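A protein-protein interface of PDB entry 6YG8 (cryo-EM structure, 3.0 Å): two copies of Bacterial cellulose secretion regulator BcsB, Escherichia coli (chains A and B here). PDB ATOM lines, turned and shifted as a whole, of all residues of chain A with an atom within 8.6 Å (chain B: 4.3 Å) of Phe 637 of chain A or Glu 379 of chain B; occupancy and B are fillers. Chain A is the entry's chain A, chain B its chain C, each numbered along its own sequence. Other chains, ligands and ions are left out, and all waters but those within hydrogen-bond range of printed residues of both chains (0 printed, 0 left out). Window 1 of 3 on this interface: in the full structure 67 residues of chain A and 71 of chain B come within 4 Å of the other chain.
Of chain B, only Gly 373, Glu 374, Lys 376, Thr 377, Tyr 378 and Glu 379 come within 4 Å of Phe 637 of chain A.
Phe 705 of chain A touches none of the printed residues of chain B.
Of the printed residues of chain A, Gly 373 of chain B touches Phe 637.
Of the printed residues of chain A, Glu 374 of chain B touches Phe 637 (3.7 Å).
Glu 379 of chain B touches just these residues of chain A: Lys 475 and Phe 637.
The nearest residue of chain A that does not touch Glu 379 of chain B is Gln 436 of chain A (6.0 Å).
No position is printed for both chains.
Of the 7 pairs that touch across the chains among the printed residues, none has its exchanged pair printed and touching as well.
Of the 15 printed residues of chain A, 2 touch a printed residue of chain B.
Hydrophobic or aromatic side chains of chain A within 4 Å of the printed part of chain B: Phe 637.
Among the printed residues, pairs that only touch across the chains: Phe 637 of chain A with Glu 374 of chain B (3.7 Å), Phe 637 of chain A with Lys 376 of chain B (3.7 Å), Phe 637 of chain A with Thr 377 of chain B (3.3 Å), Phe 637 of chain A with Tyr 378 of chain B (3.7 Å) and Phe 637 of chain A with Glu 379 of chain B (3.5 Å).
The backbone carbonyl oxygen of Lys 475 of chain A is in hydrogen-bond range of the side-chain amide nitrogen of Asn 434 of chain A (2.9 Å).
The backbone carbonyl oxygen (O) of Glu 379 of chain B lies within hydrogen-bond range of the side-chain amino group (NZ) of Lys 376 of chain B, at 3.4 Å.
The backbone NH (N) of Thr 377 of chain B sits at hydrogen-bond distance from the side-chain amide oxygen (OE1) of Gln 381 of chain B.
The side-chain carboxylate (OE2) of Glu 379 of chain B is in salt-bridge range of the side-chain amino group (NZ) of Lys 475 of chain A, 3.5 Å away.
The backbone carbonyl oxygen (O) of Gly 373 of chain B lies close to the backbone carbonyl oxygen (O) of Phe 637 of chain A.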
ATOM      1  N   ASN A 434     -27.614  -8.452 -17.984  1.00  0.00           N
ATOM      2  CA  ASN A 434     -27.434  -7.701 -16.742  1.00  0.00           C
ATOM      3  C   ASN A 434     -28.627  -6.791 -16.466  1.00  0.00           C
ATOM      4  O   ASN A 434     -28.475  -5.585 -16.272  1.00  0.00           O
ATOM      5  CB  ASN A 434     -26.138  -6.893 -16.767  1.00  0.00           C
ATOM      6  CG  ASN A 434     -24.913  -7.764 -16.700  1.00  0.00           C
ATOM      7  OD1 ASN A 434     -24.736  -8.533 -15.758  1.00  0.00           O
ATOM      8  ND2 ASN A 434     -24.056  -7.652 -17.702  1.00  0.00           N
ATOM      9  N   ASN A 435     -29.825  -7.374 -16.459  1.00  0.00           N
ATOM     10  CA  ASN A 435     -31.073  -6.671 -16.184  1.00  0.00           C
ATOM     11  C   ASN A 435     -31.338  -5.529 -17.156  1.00  0.00           C
ATOM     12  O   ASN A 435     -32.189  -4.678 -16.891  1.00  0.00           O
ATOM     13  CB  ASN A 435     -31.108  -6.142 -14.747  1.00  0.00           C
ATOM     14  CG  ASN A 435     -31.496  -7.206 -13.747  1.00  0.00           C
ATOM     15  OD1 ASN A 435     -30.661  -7.685 -12.980  1.00  0.00           O
ATOM     16  ND2 ASN A 435     -32.769  -7.580 -13.745  1.00  0.00           N
ATOM     17  N   GLN A 436     -30.632  -5.491 -18.282  1.00  0.00           N
ATOM     18  CA  GLN A 436     -30.736  -4.405 -19.242  1.00  0.00           C
ATOM     19  C   GLN A 436     -31.212  -4.954 -20.577  1.00  0.00           C
ATOM     20  O   GLN A 436     -30.526  -5.773 -21.194  1.00  0.00           O
ATOM     21  CB  GLN A 436     -29.395  -3.695 -19.401  1.00  0.00           C
ATOM     22  CG  GLN A 436     -29.418  -2.516 -20.343  1.00  0.00           C
ATOM     23  CD  GLN A 436     -28.110  -1.758 -20.333  1.00  0.00           C
ATOM     24  OE1 GLN A 436     -27.199  -2.082 -19.572  1.00  0.00           O
ATOM     25  NE2 GLN A 436     -28.008  -0.741 -21.179  1.00  0.00           N
ATOM     26  N   LYS A 475     -21.173  -2.874 -20.889  1.00  0.00           N
ATOM     27  CA  LYS A 475     -22.008  -3.440 -19.838  1.00  0.00           C
ATOM     28  C   LYS A 475     -21.732  -4.922 -19.653  1.00  0.00           C
ATOM     29  O   LYS A 475     -22.637  -5.688 -19.306  1.00  0.00           O
ATOM     30  CB  LYS A 475     -23.502  -3.219 -20.101  1.00  0.00           C
ATOM     31  CG  LYS A 475     -23.931  -1.760 -20.123  1.00  0.00           C
ATOM     32  CD  LYS A 475     -23.887  -1.136 -18.732  1.00  0.00           C
ATOM     33  CE  LYS A 475     -22.665  -0.251 -18.545  1.00  0.00           C
ATOM     34  NZ  LYS A 475     -22.656   0.406 -17.210  1.00  0.00           N
ATOM     35  N   ARG A 533     -11.725  -3.361  -9.300  1.00  0.00           N
ATOM     36  CA  ARG A 533     -12.951  -4.009  -9.731  1.00  0.00           C
ATOM     37  C   ARG A 533     -12.669  -5.332 -10.419  1.00  0.00           C
ATOM     38  O   ARG A 533     -13.545  -6.198 -10.461  1.00  0.00           O
ATOM     39  CB  ARG A 533     -13.738  -3.087 -10.667  1.00  0.00           C
ATOM     40  CG  ARG A 533     -15.096  -3.621 -11.092  1.00  0.00           C
ATOM     41  CD  ARG A 533     -16.192  -3.123 -10.176  1.00  0.00           C
ATOM     42  NE  ARG A 533     -16.593  -1.759 -10.502  1.00  0.00           N
ATOM     43  CZ  ARG A 533     -17.411  -1.025  -9.757  1.00  0.00           C
ATOM     44  NH1 ARG A 533     -17.915  -1.521  -8.637  1.00  0.00           N
ATOM     45  NH2 ARG A 533     -17.722   0.208 -10.129  1.00  0.00           N
ATOM     46  N   GLN A 634     -13.908  12.620  -9.765  1.00  0.00           N
ATOM     47  CA  GLN A 634     -14.376  11.283  -9.404  1.00  0.00           C
ATOM     48  C   GLN A 634     -15.850  11.167  -9.784  1.00  0.00           C
ATOM     49  O   GLN A 634     -16.752  11.295  -8.956  1.00  0.00           O
ATOM     50  CB  GLN A 634     -14.146  11.017  -7.920  1.00  0.00           C
ATOM     51  CG  GLN A 634     -14.508   9.608  -7.474  1.00  0.00           C
ATOM     52  CD  GLN A 634     -13.475   8.584  -7.888  1.00  0.00           C
ATOM     53  OE1 GLN A 634     -12.382   8.531  -7.328  1.00  0.00           O
ATOM     54  NE2 GLN A 634     -13.813   7.766  -8.874  1.00  0.00           N
ATOM     55  N   THR A 635     -16.087  10.923 -11.067  1.00  0.00           N
ATOM     56  CA  THR A 635     -17.445  10.762 -11.555  1.00  0.00           C
ATOM     57  C   THR A 635     -18.028   9.430 -11.082  1.00  0.00           C
ATOM     58  O   THR A 635     -17.304   8.440 -10.943  1.00  0.00           O
ATOM     59  CB  THR A 635     -17.470  10.843 -13.080  1.00  0.00           C
ATOM     60  OG1 THR A 635     -18.815  10.710 -13.556  1.00  0.00           O
ATOM     61  CG2 THR A 635     -16.594   9.765 -13.693  1.00  0.00           C
ATOM     62  N   PRO A 636     -19.334   9.384 -10.802  1.00  0.00           N
ATOM     63  CA  PRO A 636     -19.929   8.111 -10.357  1.00  0.00           C
ATOM     64  C   PRO A 636     -19.886   7.027 -11.421  1.00  0.00           C
ATOM     65  O   PRO A 636     -19.390   5.924 -11.162  1.00  0.00           O
ATOM     66  CB  PRO A 636     -21.366   8.509  -9.992  1.00  0.00           C
ATOM     67  CG  PRO A 636     -21.623   9.763 -10.757  1.00  0.00           C
ATOM     68  CD  PRO A 636     -20.313  10.483 -10.790  1.00  0.00           C
ATOM     69  N   PHE A 637     -20.390   7.314 -12.619  1.00  0.00           N
ATOM     70  CA  PHE A 637     -20.362   6.359 -13.720  1.00  0.00           C
ATOM     71  C   PHE A 637     -19.404   6.866 -14.784  1.00  0.00           C
ATOM     72  O   PHE A 637     -19.790   7.693 -15.624  1.00  0.00           O
ATOM     73  CB  PHE A 637     -21.761   6.156 -14.306  1.00  0.00           C
ATOM     74  CG  PHE A 637     -22.810   5.862 -13.277  1.00  0.00           C
ATOM     75  CD1 PHE A 637     -23.011   4.571 -12.827  1.00  0.00           C
ATOM     76  CD2 PHE A 637     -23.597   6.875 -12.761  1.00  0.00           C
ATOM     77  CE1 PHE A 637     -23.972   4.296 -11.881  1.00  0.00           C
ATOM     78  CE2 PHE A 637     -24.561   6.606 -11.813  1.00  0.00           C
ATOM     79  CZ  PHE A 637     -24.749   5.314 -11.374  1.00  0.00           C
ATOM     80  N   PRO A 638     -18.155   6.420 -14.794  1.00  0.00           N
ATOM     81  CA  PRO A 638     -17.198   6.903 -15.789  1.00  0.00           C
ATOM     82  C   PRO A 638     -17.414   6.225 -17.135  1.00  0.00           C
ATOM     83  O   PRO A 638     -18.183   5.274 -17.273  1.00  0.00           O
ATOM     84  CB  PRO A 638     -15.848   6.517 -15.187  1.00  0.00           C
ATOM     85  CG  PRO A 638     -16.149   5.279 -14.422  1.00  0.00           C
ATOM     86  CD  PRO A 638     -17.548   5.439 -13.879  1.00  0.00           C
ATOM     87  N   GLY A 639     -16.711   6.740 -18.134  1.00  0.00           N
ATOM     88  CA  GLY A 639     -16.706   6.108 -19.431  1.00  0.00           C
ATOM     89  C   GLY A 639     -15.918   4.809 -19.403  1.00  0.00           C
ATOM     90  O   GLY A 639     -15.641   4.220 -18.359  1.00  0.00           O
ATOM     91  N   ILE A 640     -15.551   4.361 -20.599  1.00  0.00           N
ATOM     92  CA  ILE A 640     -14.721   3.170 -20.739  1.00  0.00           C
ATOM     93  C   ILE A 640     -13.246   3.536 -20.790  1.00  0.00           C
ATOM     94  O   ILE A 640     -12.410   2.883 -20.159  1.00  0.00           O
ATOM     95  CB  ILE A 640     -15.154   2.365 -21.979  1.00  0.00           C
ATOM     96  CG1 ILE A 640     -16.634   2.002 -21.864  1.00  0.00           C
ATOM     97  CG2 ILE A 640     -14.315   1.105 -22.109  1.00  0.00           C
ATOM     98  CD1 ILE A 640     -16.957   1.148 -20.659  1.00  0.00           C
ATOM     99  N   ASP A 643      -9.723   8.149 -19.115  1.00  0.00           N
ATOM    100  CA  ASP A 643      -9.677   9.620 -19.105  1.00  0.00           C
ATOM    101  C   ASP A 643      -8.688  10.161 -18.070  1.00  0.00           C
ATOM    102  O   ASP A 643      -9.043  10.830 -17.100  1.00  0.00           O
ATOM    103  CB  ASP A 643     -11.081  10.232 -18.944  1.00  0.00           C
ATOM    104  CG  ASP A 643     -11.762   9.901 -17.616  1.00  0.00           C
ATOM    105  OD1 ASP A 643     -11.190   9.208 -16.758  1.00  0.00           O
ATOM    106  OD2 ASP A 643     -12.912  10.348 -17.431  1.00  0.00           O
ATOM    107  N   PHE A 705     -13.228  -0.457  -6.420  1.00  0.00           N
ATOM    108  CA  PHE A 705     -12.802  -0.131  -7.774  1.00  0.00           C
ATOM    109  C   PHE A 705     -11.626   0.830  -7.685  1.00  0.00           C
ATOM    110  O   PHE A 705     -11.127   1.132  -6.599  1.00  0.00           O
ATOM    111  CB  PHE A 705     -13.950   0.453  -8.607  1.00  0.00           C
ATOM    112  CG  PHE A 705     -14.616   1.649  -7.989  1.00  0.00           C
ATOM    113  CD1 PHE A 705     -14.052   2.908  -8.094  1.00  0.00           C
ATOM    114  CD2 PHE A 705     -15.824   1.519  -7.332  1.00  0.00           C
ATOM    115  CE1 PHE A 705     -14.668   4.005  -7.536  1.00  0.00           C
ATOM    116  CE2 PHE A 705     -16.446   2.615  -6.775  1.00  0.00           C
ATOM    117  CZ  PHE A 705     -15.866   3.860  -6.878  1.00  0.00           C
ATOM    118  N   ARG A 720     -10.519   6.224  -8.129  1.00  0.00           N
ATOM    119  CA  ARG A 720      -9.830   6.068  -9.410  1.00  0.00           C
ATOM    120  C   ARG A 720      -8.822   7.200  -9.525  1.00  0.00           C
ATOM    121  O   ARG A 720      -9.116   8.270 -10.055  1.00  0.00           O
ATOM    122  CB  ARG A 720     -10.814   6.093 -10.570  1.00  0.00           C
ATOM    123  CG  ARG A 720     -11.864   5.009 -10.534  1.00  0.00           C
ATOM    124  CD  ARG A 720     -12.566   4.903 -11.870  1.00  0.00           C
ATOM    125  NE  ARG A 720     -13.659   3.941 -11.833  1.00  0.00           N
ATOM    126  CZ  ARG A 720     -14.891   4.231 -11.431  1.00  0.00           C
ATOM    127  NH1 ARG A 720     -15.185   5.460 -11.033  1.00  0.00           N
ATOM    128  NH2 ARG A 720     -15.828   3.294 -11.430  1.00  0.00           N
ATOM    129  N   GLY B 373     -23.790   7.967 -20.460  1.00  0.00           N
ATOM    130  CA  GLY B 373     -23.383   7.224 -19.283  1.00  0.00           C
ATOM    131  C   GLY B 373     -22.739   8.079 -18.216  1.00  0.00           C
ATOM    132  O   GLY B 373     -22.640   7.643 -17.065  1.00  0.00           O
ATOM    133  N   GLU B 374     -22.300   9.283 -18.568  1.00  0.00           N
ATOM    134  CA  GLU B 374     -21.746  10.208 -17.592  1.00  0.00           C
ATOM    135  C   GLU B 374     -22.768  11.211 -17.089  1.00  0.00           C
ATOM    136  O   GLU B 374     -22.556  11.815 -16.032  1.00  0.00           O
ATOM    137  CB  GLU B 374     -20.554  10.955 -18.189  1.00  0.00           C
ATOM    138  CG  GLU B 374     -19.623  10.073 -18.993  1.00  0.00           C
ATOM    139  CD  GLU B 374     -18.346  10.784 -19.385  1.00  0.00           C
ATOM    140  OE1 GLU B 374     -17.780  11.506 -18.538  1.00  0.00           O
ATOM    141  OE2 GLU B 374     -17.906  10.620 -20.542  1.00  0.00           O
ATOM    142  N   LYS B 376     -25.744  10.298 -16.208  1.00  0.00           N
ATOM    143  CA  LYS B 376     -26.623   9.576 -15.304  1.00  0.00           C
ATOM    144  C   LYS B 376     -26.320   9.927 -13.855  1.00  0.00           C
ATOM    145  O   LYS B 376     -25.177  10.198 -13.481  1.00  0.00           O
ATOM    146  CB  LYS B 376     -26.472   8.069 -15.492  1.00  0.00           C
ATOM    147  CG  LYS B 376     -26.906   7.554 -16.837  1.00  0.00           C
ATOM    148  CD  LYS B 376     -27.071   6.050 -16.800  1.00  0.00           C
ATOM    149  CE  LYS B 376     -25.834   5.372 -16.252  1.00  0.00           C
ATOM    150  NZ  LYS B 376     -25.922   3.896 -16.399  1.00  0.00           N
ATOM    151  N   THR B 377     -27.366   9.916 -13.036  1.00  0.00           N
ATOM    152  CA  THR B 377     -27.232  10.026 -11.591  1.00  0.00           C
ATOM    153  C   THR B 377     -27.347   8.677 -10.901  1.00  0.00           C
ATOM    154  O   THR B 377     -26.582   8.389  -9.976  1.00  0.00           O
ATOM    155  CB  THR B 377     -28.290  10.979 -11.034  1.00  0.00           C
ATOM    156  OG1 THR B 377     -29.580  10.600 -11.527  1.00  0.00           O
ATOM    157  CG2 THR B 377     -27.994  12.399 -11.472  1.00  0.00           C
ATOM    158  N   TYR B 378     -28.283   7.842 -11.340  1.00  0.00           N
ATOM    159  CA  TYR B 378     -28.373   6.453 -10.920  1.00  0.00           C
ATOM    160  C   TYR B 378     -28.355   5.576 -12.160  1.00  0.00           C
ATOM    161  O   TYR B 378     -28.610   6.039 -13.273  1.00  0.00           O
ATOM    162  CB  TYR B 378     -29.627   6.184 -10.076  1.00  0.00           C
ATOM    163  CG  TYR B 378     -30.936   6.565 -10.726  1.00  0.00           C
ATOM    164  CD1 TYR B 378     -31.308   7.894 -10.857  1.00  0.00           C
ATOM    165  CD2 TYR B 378     -31.812   5.596 -11.184  1.00  0.00           C
ATOM    166  CE1 TYR B 378     -32.503   8.246 -11.438  1.00  0.00           C
ATOM    167  CE2 TYR B 378     -33.012   5.941 -11.766  1.00  0.00           C
ATOM    168  CZ  TYR B 378     -33.352   7.265 -11.893  1.00  0.00           C
ATOM    169  OH  TYR B 378     -34.549   7.610 -12.475  1.00  0.00           O
ATOM    170  N   GLU B 379     -28.039   4.298 -11.966  1.00  0.00           N
ATOM    171  CA  GLU B 379     -27.728   3.448 -13.111  1.00  0.00           C
ATOM    172  C   GLU B 379     -28.980   3.073 -13.894  1.00  0.00           C
ATOM    173  O   GLU B 379     -28.976   3.079 -15.129  1.00  0.00           O
ATOM    174  CB  GLU B 379     -26.977   2.201 -12.655  1.00  0.00           C
ATOM    175  CG  GLU B 379     -26.567   1.306 -13.808  1.00  0.00           C
ATOM    176  CD  GLU B 379     -25.309   0.523 -13.517  1.00  0.00           C
ATOM    177  OE1 GLU B 379     -24.858   0.538 -12.354  1.00  0.00           O
ATOM    178  OE2 GLU B 379     -24.767  -0.100 -14.455  1.00  0.00           O
ATOM    179  N   GLU B 380     -30.064   2.740 -13.195  1.00  0.00           N
ATOM    180  CA  GLU B 380     -31.309   2.360 -13.865  1.00  0.00           C
ATOM    181  C   GLU B 380     -32.104   3.622 -14.221  1.00  0.00           C
ATOM    182  O   GLU B 380     -33.290   3.770 -13.922  1.00  0.00           O
ATOM    183  CB  GLU B 380     -32.106   1.405 -12.988  1.00  0.00           C
ATOM    184  CG  GLU B 380     -33.304   0.774 -13.683  1.00  0.00           C
ATOM    185  CD  GLU B 380     -32.919  -0.380 -14.585  1.00  0.00           C
ATOM    186  OE1 GLU B 380     -31.795  -0.906 -14.439  1.00  0.00           O
ATOM    187  OE2 GLU B 380     -33.734  -0.755 -15.453  1.00  0.00           O
ATOM    188  N   GLN B 381     -31.417   4.546 -14.893  1.00  0.00           N
ATOM    189  CA  GLN B 381     -32.009   5.810 -15.307  1.00  0.00           C
ATOM    190  C   GLN B 381     -32.371   5.876 -16.778  1.00  0.00           C
ATOM    191  O   GLN B 381     -33.427   6.424 -17.107  1.00  0.00           O
ATOM    192  CB  GLN B 381     -31.062   6.979 -15.003  1.00  0.00           C
ATOM    193  CG  GLN B 381     -31.672   8.344 -15.241  1.00  0.00           C
ATOM    194  CD  GLN B 381     -30.678   9.457 -15.032  1.00  0.00           C
ATOM    195  OE1 GLN B 381     -29.732   9.319 -14.263  1.00  0.00           O
ATOM    196  NE2 GLN B 381     -30.883  10.570 -15.719  1.00  0.00           N
ATOM    197  N   LEU B 382     -31.538   5.341 -17.666  1.00  0.00           N
ATOM    198  CA  LEU B 382     -31.743   5.453 -19.102  1.00  0.00           C
ATOM    199  C   LEU B 382     -32.579   4.316 -19.662  1.00  0.00           C
ATOM    200  O   LEU B 382     -32.430   3.971 -20.838  1.00  0.00           O
ATOM    201  CB  LEU B 382     -30.397   5.510 -19.820  1.00  0.00           C
ATOM    202  CG  LEU B 382     -29.504   6.681 -19.433  1.00  0.00           C
ATOM    203  CD1 LEU B 382     -28.246   6.686 -20.267  1.00  0.00           C
ATOM    204  CD2 LEU B 382     -30.259   7.980 -19.596  1.00  0.00           C
